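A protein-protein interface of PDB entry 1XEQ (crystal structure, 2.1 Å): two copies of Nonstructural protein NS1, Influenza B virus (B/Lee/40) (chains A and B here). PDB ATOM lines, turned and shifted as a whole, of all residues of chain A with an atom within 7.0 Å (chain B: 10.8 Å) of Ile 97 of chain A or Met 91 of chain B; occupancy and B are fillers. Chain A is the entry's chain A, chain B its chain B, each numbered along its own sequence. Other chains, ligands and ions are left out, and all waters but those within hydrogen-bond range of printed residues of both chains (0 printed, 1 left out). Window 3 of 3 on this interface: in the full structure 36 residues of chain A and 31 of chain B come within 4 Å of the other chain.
Glu 29 of chain A touches Asp 92 of chain B. Pro 93 of chain B touches Glu 29 of chain A. Arg 33 of chain A touches Met 91 of chain B (CD to O, 3.5 Å). Trp 36 of chain A touches Pro 93 of chain B. Lys 86 of chain A touches Phe 90 of chain B (CE to CE2, 3.5 Å). CE2 of Phe 90 of chain B touches O of Ser 94 of chain A (3.7 Å). Phe 90 of chain B touches Gly 96 of chain A. SD of Met 91 of chain B touches CD1 of Ile 97 of chain A (3.6 Å). NZ of Lys 86 of chain B touches CZ of Phe 100 of chain A, 3.6 Å away. CZ of Phe 100 of chain A touches CG of Phe 90 of chain B, 3.6 Å away.
Hydrophobic or aromatic side chains of chain A within 4 Å of the printed part of chain B: Trp 36, Ile 97 and Phe 100.
The backbone carbonyl oxygen (O) of Leu 88 of chain B lies within hydrogen-bond range of the guanidinium group (NH1) of Arg 33 of chain A, 2.8 Å away. O of Leu 89 of chain B is in hydrogen-bond range of NH1 of Arg 33 of chain A (3.1 Å). NH2 of Arg 33 of chain A lies within salt-bridge range of OD1 of Asp 92 of chain B (3.4 Å). O of Leu 89 of chain B lies close to NZ of Lys 86 of chain A, at 3.1 Å. The backbone NH (N) of Ile 97 of chain A lies within hydrogen-bond range of the backbone carbonyl oxygen (O) of Phe 90 of chain B.
Of the printed residues of chain B, Arg 33 of chain A touches Leu 88 (2.8 Å), Leu 89 (3.1 Å), Met 91 (3.5 Å), Asp 92 (3.2 Å) and Pro 93 (3.7 Å). No residue of chain B comes within 4 Å of Ala 95 of chain A. Gly 96 of chain A touches one residue of chain B. Of chain B, only Phe 90 and Met 91 come within 4 Å of Ile 97 of chain A. No residue of chain B comes within 4 Å of Glu 98 of chain A. No residue of chain B comes within 4 Å of Gly 99 of chain A. Of the printed residues of chain B, Phe 100 of chain A touches Lys 86 and Phe 90. Met 85 of chain B touches none of the printed residues of chain A. Val 87 of chain B touches none of the printed residues of chain A. Met 91 of chain B touches three residues of chain A. The nearest residue of chain B that does not touch Ile 97 of chain A is Asp 92 of chain B (6.1 Å). The nearest residue of chain A that does not touch Met 91 of chain B is Gly 96 of chain A (5.5 Å). The nearest printed residue of chain A that does not touch Leu 88 of chain B is Trp 36 of chain A (5.9 Å).
NE of Arg 33 of chain A lies within salt-bridge range of OE1 of Glu 29 of chain A (2.8 Å). The side-chain amino group of Lys 86 of chain A sits at hydrogen-bond distance from the backbone carbonyl oxygen of Ser 94 of chain A. The side-chain hydroxyl (OG) of Ser 94 of chain A sits at hydrogen-bond distance from the backbone carbonyl oxygen (O) of Glu 98 of chain A, 3.2 Å away.
Position printed for both chains: 86.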
ATOM      1  N   GLU A  29     -15.520  34.083  18.832  1.00  0.00           N
ATOM      2  CA  GLU A  29     -16.132  33.880  20.130  1.00  0.00           C
ATOM      3  C   GLU A  29     -15.921  32.456  20.630  1.00  0.00           C
ATOM      4  O   GLU A  29     -15.670  32.237  21.803  1.00  0.00           O
ATOM      5  CB  GLU A  29     -17.640  34.282  20.054  1.00  0.00           C
ATOM      6  CG  GLU A  29     -18.479  34.001  21.273  1.00  0.00           C
ATOM      7  CD  GLU A  29     -18.066  34.816  22.475  1.00  0.00           C
ATOM      8  OE1 GLU A  29     -18.374  34.395  23.609  1.00  0.00           O
ATOM      9  OE2 GLU A  29     -17.416  35.870  22.288  1.00  0.00           O
ATOM     10  N   ARG A  33     -14.013  31.310  23.970  1.00  0.00           N
ATOM     11  CA  ARG A  33     -14.614  30.395  24.948  1.00  0.00           C
ATOM     12  C   ARG A  33     -13.746  29.200  25.195  1.00  0.00           C
ATOM     13  O   ARG A  33     -13.631  28.748  26.311  1.00  0.00           O
ATOM     14  CB  ARG A  33     -15.983  29.944  24.503  1.00  0.00           C
ATOM     15  CG  ARG A  33     -17.022  31.067  24.482  1.00  0.00           C
ATOM     16  CD  ARG A  33     -18.394  30.603  24.098  1.00  0.00           C
ATOM     17  NE  ARG A  33     -19.294  31.732  23.914  1.00  0.00           N
ATOM     18  CZ  ARG A  33     -20.635  31.643  23.707  1.00  0.00           C
ATOM     19  NH1 ARG A  33     -21.299  30.490  23.687  1.00  0.00           N
ATOM     20  NH2 ARG A  33     -21.337  32.741  23.571  1.00  0.00           N
ATOM     21  N   TRP A  36     -10.662  30.358  27.324  1.00  0.00           N
ATOM     22  CA  TRP A  36     -11.125  30.547  28.678  1.00  0.00           C
ATOM     23  C   TRP A  36     -11.138  29.219  29.445  1.00  0.00           C
ATOM     24  O   TRP A  36     -10.843  29.144  30.587  1.00  0.00           O
ATOM     25  CB  TRP A  36     -12.558  31.096  28.519  1.00  0.00           C
ATOM     26  CG  TRP A  36     -13.486  31.088  29.606  1.00  0.00           C
ATOM     27  CD1 TRP A  36     -13.225  31.402  30.894  1.00  0.00           C
ATOM     28  CD2 TRP A  36     -14.949  30.847  29.524  1.00  0.00           C
ATOM     29  NE1 TRP A  36     -14.394  31.335  31.616  1.00  0.00           N
ATOM     30  CE2 TRP A  36     -15.453  30.991  30.791  1.00  0.00           C
ATOM     31  CE3 TRP A  36     -15.825  30.464  28.500  1.00  0.00           C
ATOM     32  CZ2 TRP A  36     -16.823  30.848  31.080  1.00  0.00           C
ATOM     33  CZ3 TRP A  36     -17.212  30.362  28.744  1.00  0.00           C
ATOM     34  CH2 TRP A  36     -17.694  30.546  30.032  1.00  0.00           C
ATOM     35  N   LYS A  86     -24.622  27.567  15.308  1.00  0.00           N
ATOM     36  CA  LYS A  86     -25.575  26.598  15.861  1.00  0.00           C
ATOM     37  C   LYS A  86     -26.423  25.937  14.748  1.00  0.00           C
ATOM     38  O   LYS A  86     -26.559  24.696  14.672  1.00  0.00           O
ATOM     39  CB  LYS A  86     -26.466  27.233  16.916  1.00  0.00           C
ATOM     40  CG  LYS A  86     -25.690  27.439  18.210  1.00  0.00           C
ATOM     41  CD  LYS A  86     -26.398  28.474  19.120  1.00  0.00           C
ATOM     42  CE  LYS A  86     -25.629  28.614  20.410  1.00  0.00           C
ATOM     43  NZ  LYS A  86     -26.168  29.666  21.378  1.00  0.00           N
ATOM     44  N   SER A  94     -30.878  29.206  19.892  1.00  0.00           N
ATOM     45  CA  SER A  94     -31.130  30.223  20.873  1.00  0.00           C
ATOM     46  C   SER A  94     -29.867  30.533  21.664  1.00  0.00           C
ATOM     47  O   SER A  94     -29.106  29.625  22.007  1.00  0.00           O
ATOM     48  CB  SER A  94     -32.271  29.809  21.828  1.00  0.00           C
ATOM     49  OG  SER A  94     -31.923  28.625  22.484  1.00  0.00           O
ATOM     50  N   ALA A  95     -29.668  31.814  22.021  1.00  0.00           N
ATOM     51  CA  ALA A  95     -28.501  32.208  22.864  1.00  0.00           C
ATOM     52  C   ALA A  95     -28.544  31.486  24.170  1.00  0.00           C
ATOM     53  O   ALA A  95     -29.597  31.191  24.660  1.00  0.00           O
ATOM     54  CB  ALA A  95     -28.507  33.757  23.110  1.00  0.00           C
ATOM     55  N   GLY A  96     -27.391  31.146  24.734  1.00  0.00           N
ATOM     56  CA  GLY A  96     -27.355  30.747  26.142  1.00  0.00           C
ATOM     57  C   GLY A  96     -27.833  29.328  26.360  1.00  0.00           C
ATOM     58  O   GLY A  96     -28.310  28.643  25.421  1.00  0.00           O
ATOM     59  N   ILE A  97     -27.777  28.913  27.618  1.00  0.00           N
ATOM     60  CA  ILE A  97     -28.098  27.522  27.963  1.00  0.00           C
ATOM     61  C   ILE A  97     -29.595  27.288  28.040  1.00  0.00           C
ATOM     62  O   ILE A  97     -30.058  26.143  27.965  1.00  0.00           O
ATOM     63  CB  ILE A  97     -27.481  27.225  29.322  1.00  0.00           C
ATOM     64  CG1 ILE A  97     -27.590  25.704  29.643  1.00  0.00           C
ATOM     65  CG2 ILE A  97     -28.173  28.047  30.417  1.00  0.00           C
ATOM     66  CD1 ILE A  97     -26.627  25.322  30.779  1.00  0.00           C
ATOM     67  N   GLU A  98     -30.370  28.385  28.139  1.00  0.00           N
ATOM     68  CA  GLU A  98     -31.840  28.298  28.093  1.00  0.00           C
ATOM     69  C   GLU A  98     -32.346  28.182  26.639  1.00  0.00           C
ATOM     70  O   GLU A  98     -31.757  28.722  25.711  1.00  0.00           O
ATOM     71  CB  GLU A  98     -32.526  29.567  28.722  1.00  0.00           C
ATOM     72  CG  GLU A  98     -32.193  29.763  30.184  1.00  0.00           C
ATOM     73  CD  GLU A  98     -32.650  31.154  30.736  1.00  0.00           C
ATOM     74  OE1 GLU A  98     -33.362  31.901  30.074  1.00  0.00           O
ATOM     75  OE2 GLU A  98     -32.231  31.483  31.823  1.00  0.00           O
ATOM     76  N   GLY A  99     -33.467  27.555  26.476  1.00  0.00           N
ATOM     77  CA  GLY A  99     -34.120  27.494  25.195  1.00  0.00           C
ATOM     78  C   GLY A  99     -34.144  26.143  24.489  1.00  0.00           C
ATOM     79  O   GLY A  99     -34.770  26.047  23.465  1.00  0.00           O
ATOM     80  N   PHE A 100     -33.540  25.092  25.038  1.00  0.00           N
ATOM     81  CA  PHE A 100     -33.595  23.773  24.372  1.00  0.00           C
ATOM     82  C   PHE A 100     -35.006  23.246  24.320  1.00  0.00           C
ATOM     83  O   PHE A 100     -35.788  23.452  25.234  1.00  0.00           O
ATOM     84  CB  PHE A 100     -32.697  22.756  25.043  1.00  0.00           C
ATOM     85  CG  PHE A 100     -31.255  23.033  24.892  1.00  0.00           C
ATOM     86  CD1 PHE A 100     -30.432  23.093  26.003  1.00  0.00           C
ATOM     87  CD2 PHE A 100     -30.680  23.041  23.671  1.00  0.00           C
ATOM     88  CE1 PHE A 100     -29.101  23.344  25.887  1.00  0.00           C
ATOM     89  CE2 PHE A 100     -29.327  23.242  23.553  1.00  0.00           C
ATOM     90  CZ  PHE A 100     -28.541  23.382  24.607  1.00  0.00           C
ATOM     91  N   LYS B  83     -18.471  17.934  19.015  1.00  0.00           N
ATOM     92  CA  LYS B  83     -18.943  17.698  20.393  1.00  0.00           C
ATOM     93  C   LYS B  83     -18.545  18.808  21.348  1.00  0.00           C
ATOM     94  O   LYS B  83     -19.359  19.289  22.216  1.00  0.00           O
ATOM     95  CB  LYS B  83     -18.473  16.331  20.957  1.00  0.00           C
ATOM     96  CG  LYS B  83     -19.181  15.103  20.369  1.00  0.00           C
ATOM     97  CD  LYS B  83     -18.752  13.800  21.072  1.00  0.00           C
ATOM     98  CE  LYS B  83     -19.525  12.537  20.571  1.00  0.00           C
ATOM     99  NZ  LYS B  83     -18.952  11.263  21.192  1.00  0.00           N
ATOM    100  N   MET B  84     -17.274  19.181  21.270  1.00  0.00           N
ATOM    101  CA  MET B  84     -16.811  20.315  22.043  1.00  0.00           C
ATOM    102  C   MET B  84     -17.537  21.623  21.678  1.00  0.00           C
ATOM    103  O   MET B  84     -17.972  22.363  22.549  1.00  0.00           O
ATOM    104  CB  MET B  84     -15.299  20.479  21.854  1.00  0.00           C
ATOM    105  CG  MET B  84     -14.530  19.356  22.319  1.00  0.00           C
ATOM    106  SD  MET B  84     -12.747  19.648  22.710  1.00  0.00           S
ATOM    107  CE  MET B  84     -12.265  19.682  21.177  1.00  0.00           C
ATOM    108  N   MET B  85     -17.713  21.869  20.397  1.00  0.00           N
ATOM    109  CA  MET B  85     -18.487  23.027  19.948  1.00  0.00           C
ATOM    110  C   MET B  85     -19.925  23.093  20.531  1.00  0.00           C
ATOM    111  O   MET B  85     -20.364  24.181  20.963  1.00  0.00           O
ATOM    112  CB  MET B  85     -18.493  23.078  18.413  1.00  0.00           C
ATOM    113  CG  MET B  85     -18.433  24.427  17.861  1.00  0.00           C
ATOM    114  SD  MET B  85     -16.782  25.202  18.271  1.00  0.00           S
ATOM    115  CE  MET B  85     -15.676  24.144  17.256  1.00  0.00           C
ATOM    116  N   LYS B  86     -20.618  21.986  20.748  1.00  0.00           N
ATOM    117  CA  LYS B  86     -21.934  22.114  21.460  1.00  0.00           C
ATOM    118  C   LYS B  86     -21.843  22.616  22.853  1.00  0.00           C
ATOM    119  O   LYS B  86     -22.649  23.457  23.318  1.00  0.00           O
ATOM    120  CB  LYS B  86     -22.677  20.877  21.628  1.00  0.00           C
ATOM    121  CG  LYS B  86     -24.086  21.286  22.189  1.00  0.00           C
ATOM    122  CD  LYS B  86     -24.598  20.530  23.375  1.00  0.00           C
ATOM    123  CE  LYS B  86     -26.063  20.907  23.513  1.00  0.00           C
ATOM    124  NZ  LYS B  86     -26.824  20.195  24.649  1.00  0.00           N
ATOM    125  N   VAL B  87     -20.867  22.182  23.560  1.00  0.00           N
ATOM    126  CA  VAL B  87     -20.760  22.612  24.902  1.00  0.00           C
ATOM    127  C   VAL B  87     -20.454  24.137  24.927  1.00  0.00           C
ATOM    128  O   VAL B  87     -20.961  24.923  25.777  1.00  0.00           O
ATOM    129  CB  VAL B  87     -19.646  21.791  25.574  1.00  0.00           C
ATOM    130  CG1 VAL B  87     -19.354  22.293  26.918  1.00  0.00           C
ATOM    131  CG2 VAL B  87     -20.050  20.349  25.611  1.00  0.00           C
ATOM    132  N   LEU B  88     -19.469  24.512  24.121  1.00  0.00           N
ATOM    133  CA  LEU B  88     -19.010  25.835  24.094  1.00  0.00           C
ATOM    134  C   LEU B  88     -20.089  26.827  23.619  1.00  0.00           C
ATOM    135  O   LEU B  88     -20.190  27.964  24.121  1.00  0.00           O
ATOM    136  CB  LEU B  88     -17.876  25.879  23.059  1.00  0.00           C
ATOM    137  CG  LEU B  88     -16.456  26.059  23.261  1.00  0.00           C
ATOM    138  CD1 LEU B  88     -15.901  25.944  24.735  1.00  0.00           C
ATOM    139  CD2 LEU B  88     -15.661  25.320  22.156  1.00  0.00           C
ATOM    140  N   LEU B  89     -20.813  26.424  22.595  1.00  0.00           N
ATOM    141  CA  LEU B  89     -21.797  27.237  21.950  1.00  0.00           C
ATOM    142  C   LEU B  89     -22.925  27.615  22.846  1.00  0.00           C
ATOM    143  O   LEU B  89     -23.527  28.633  22.603  1.00  0.00           O
ATOM    144  CB  LEU B  89     -22.380  26.620  20.657  1.00  0.00           C
ATOM    145  CG  LEU B  89     -21.446  26.829  19.492  1.00  0.00           C
ATOM    146  CD1 LEU B  89     -21.802  25.821  18.387  1.00  0.00           C
ATOM    147  CD2 LEU B  89     -21.455  28.248  18.921  1.00  0.00           C
ATOM    148  N   PHE B  90     -23.143  26.859  23.920  1.00  0.00           N
ATOM    149  CA  PHE B  90     -24.230  27.132  24.819  1.00  0.00           C
ATOM    150  C   PHE B  90     -23.866  27.607  26.209  1.00  0.00           C
ATOM    151  O   PHE B  90     -24.740  27.664  27.085  1.00  0.00           O
ATOM    152  CB  PHE B  90     -25.125  25.900  24.911  1.00  0.00           C
ATOM    153  CG  PHE B  90     -25.878  25.671  23.652  1.00  0.00           C
ATOM    154  CD1 PHE B  90     -25.380  24.776  22.722  1.00  0.00           C
ATOM    155  CD2 PHE B  90     -27.006  26.432  23.326  1.00  0.00           C
ATOM    156  CE1 PHE B  90     -26.065  24.555  21.492  1.00  0.00           C
ATOM    157  CE2 PHE B  90     -27.649  26.234  22.097  1.00  0.00           C
ATOM    158  CZ  PHE B  90     -27.180  25.323  21.201  1.00  0.00           C
ATOM    159  N   MET B  91     -22.579  27.840  26.434  1.00  0.00           N
ATOM    160  CA  MET B  91     -22.134  28.386  27.685  1.00  0.00           C
ATOM    161  C   MET B  91     -21.344  29.702  27.343  1.00  0.00           C
ATOM    162  O   MET B  91     -20.164  29.569  26.983  1.00  0.00           O
ATOM    163  CB  MET B  91     -21.260  27.389  28.405  1.00  0.00           C
ATOM    164  CG  MET B  91     -21.903  26.062  28.907  1.00  0.00           C
ATOM    165  SD  MET B  91     -23.100  25.851  30.468  1.00  0.00           S
ATOM    166  CE  MET B  91     -21.827  26.092  31.861  1.00  0.00           C
ATOM    167  N   ASP B  92     -22.060  30.885  27.374  1.00  0.00           N
ATOM    168  CA  ASP B  92     -21.591  32.323  27.013  1.00  0.00           C
ATOM    169  C   ASP B  92     -21.040  33.129  28.167  1.00  0.00           C
ATOM    170  O   ASP B  92     -21.793  33.385  29.113  1.00  0.00           O
ATOM    171  CB  ASP B  92     -22.789  33.161  26.419  1.00  0.00           C
ATOM    172  CG  ASP B  92     -22.415  34.667  26.097  1.00  0.00           C
ATOM    173  OD1 ASP B  92     -21.198  35.008  26.036  1.00  0.00           O
ATOM    174  OD2 ASP B  92     -23.258  35.580  25.913  1.00  0.00           O
ATOM    175  N   PRO B  93     -19.765  33.529  28.189  1.00  0.00           N
ATOM    176  CA  PRO B  93     -19.260  34.066  29.458  1.00  0.00           C
ATOM    177  C   PRO B  93     -19.587  35.550  29.798  1.00  0.00           C
ATOM    178  O   PRO B  93     -20.067  36.190  28.831  1.00  0.00           O
ATOM    179  CB  PRO B  93     -17.771  33.738  29.428  1.00  0.00           C
ATOM    180  CG  PRO B  93     -17.422  33.697  27.927  1.00  0.00           C
ATOM    181  CD  PRO B  93     -18.702  33.394  27.196  1.00  0.00           C
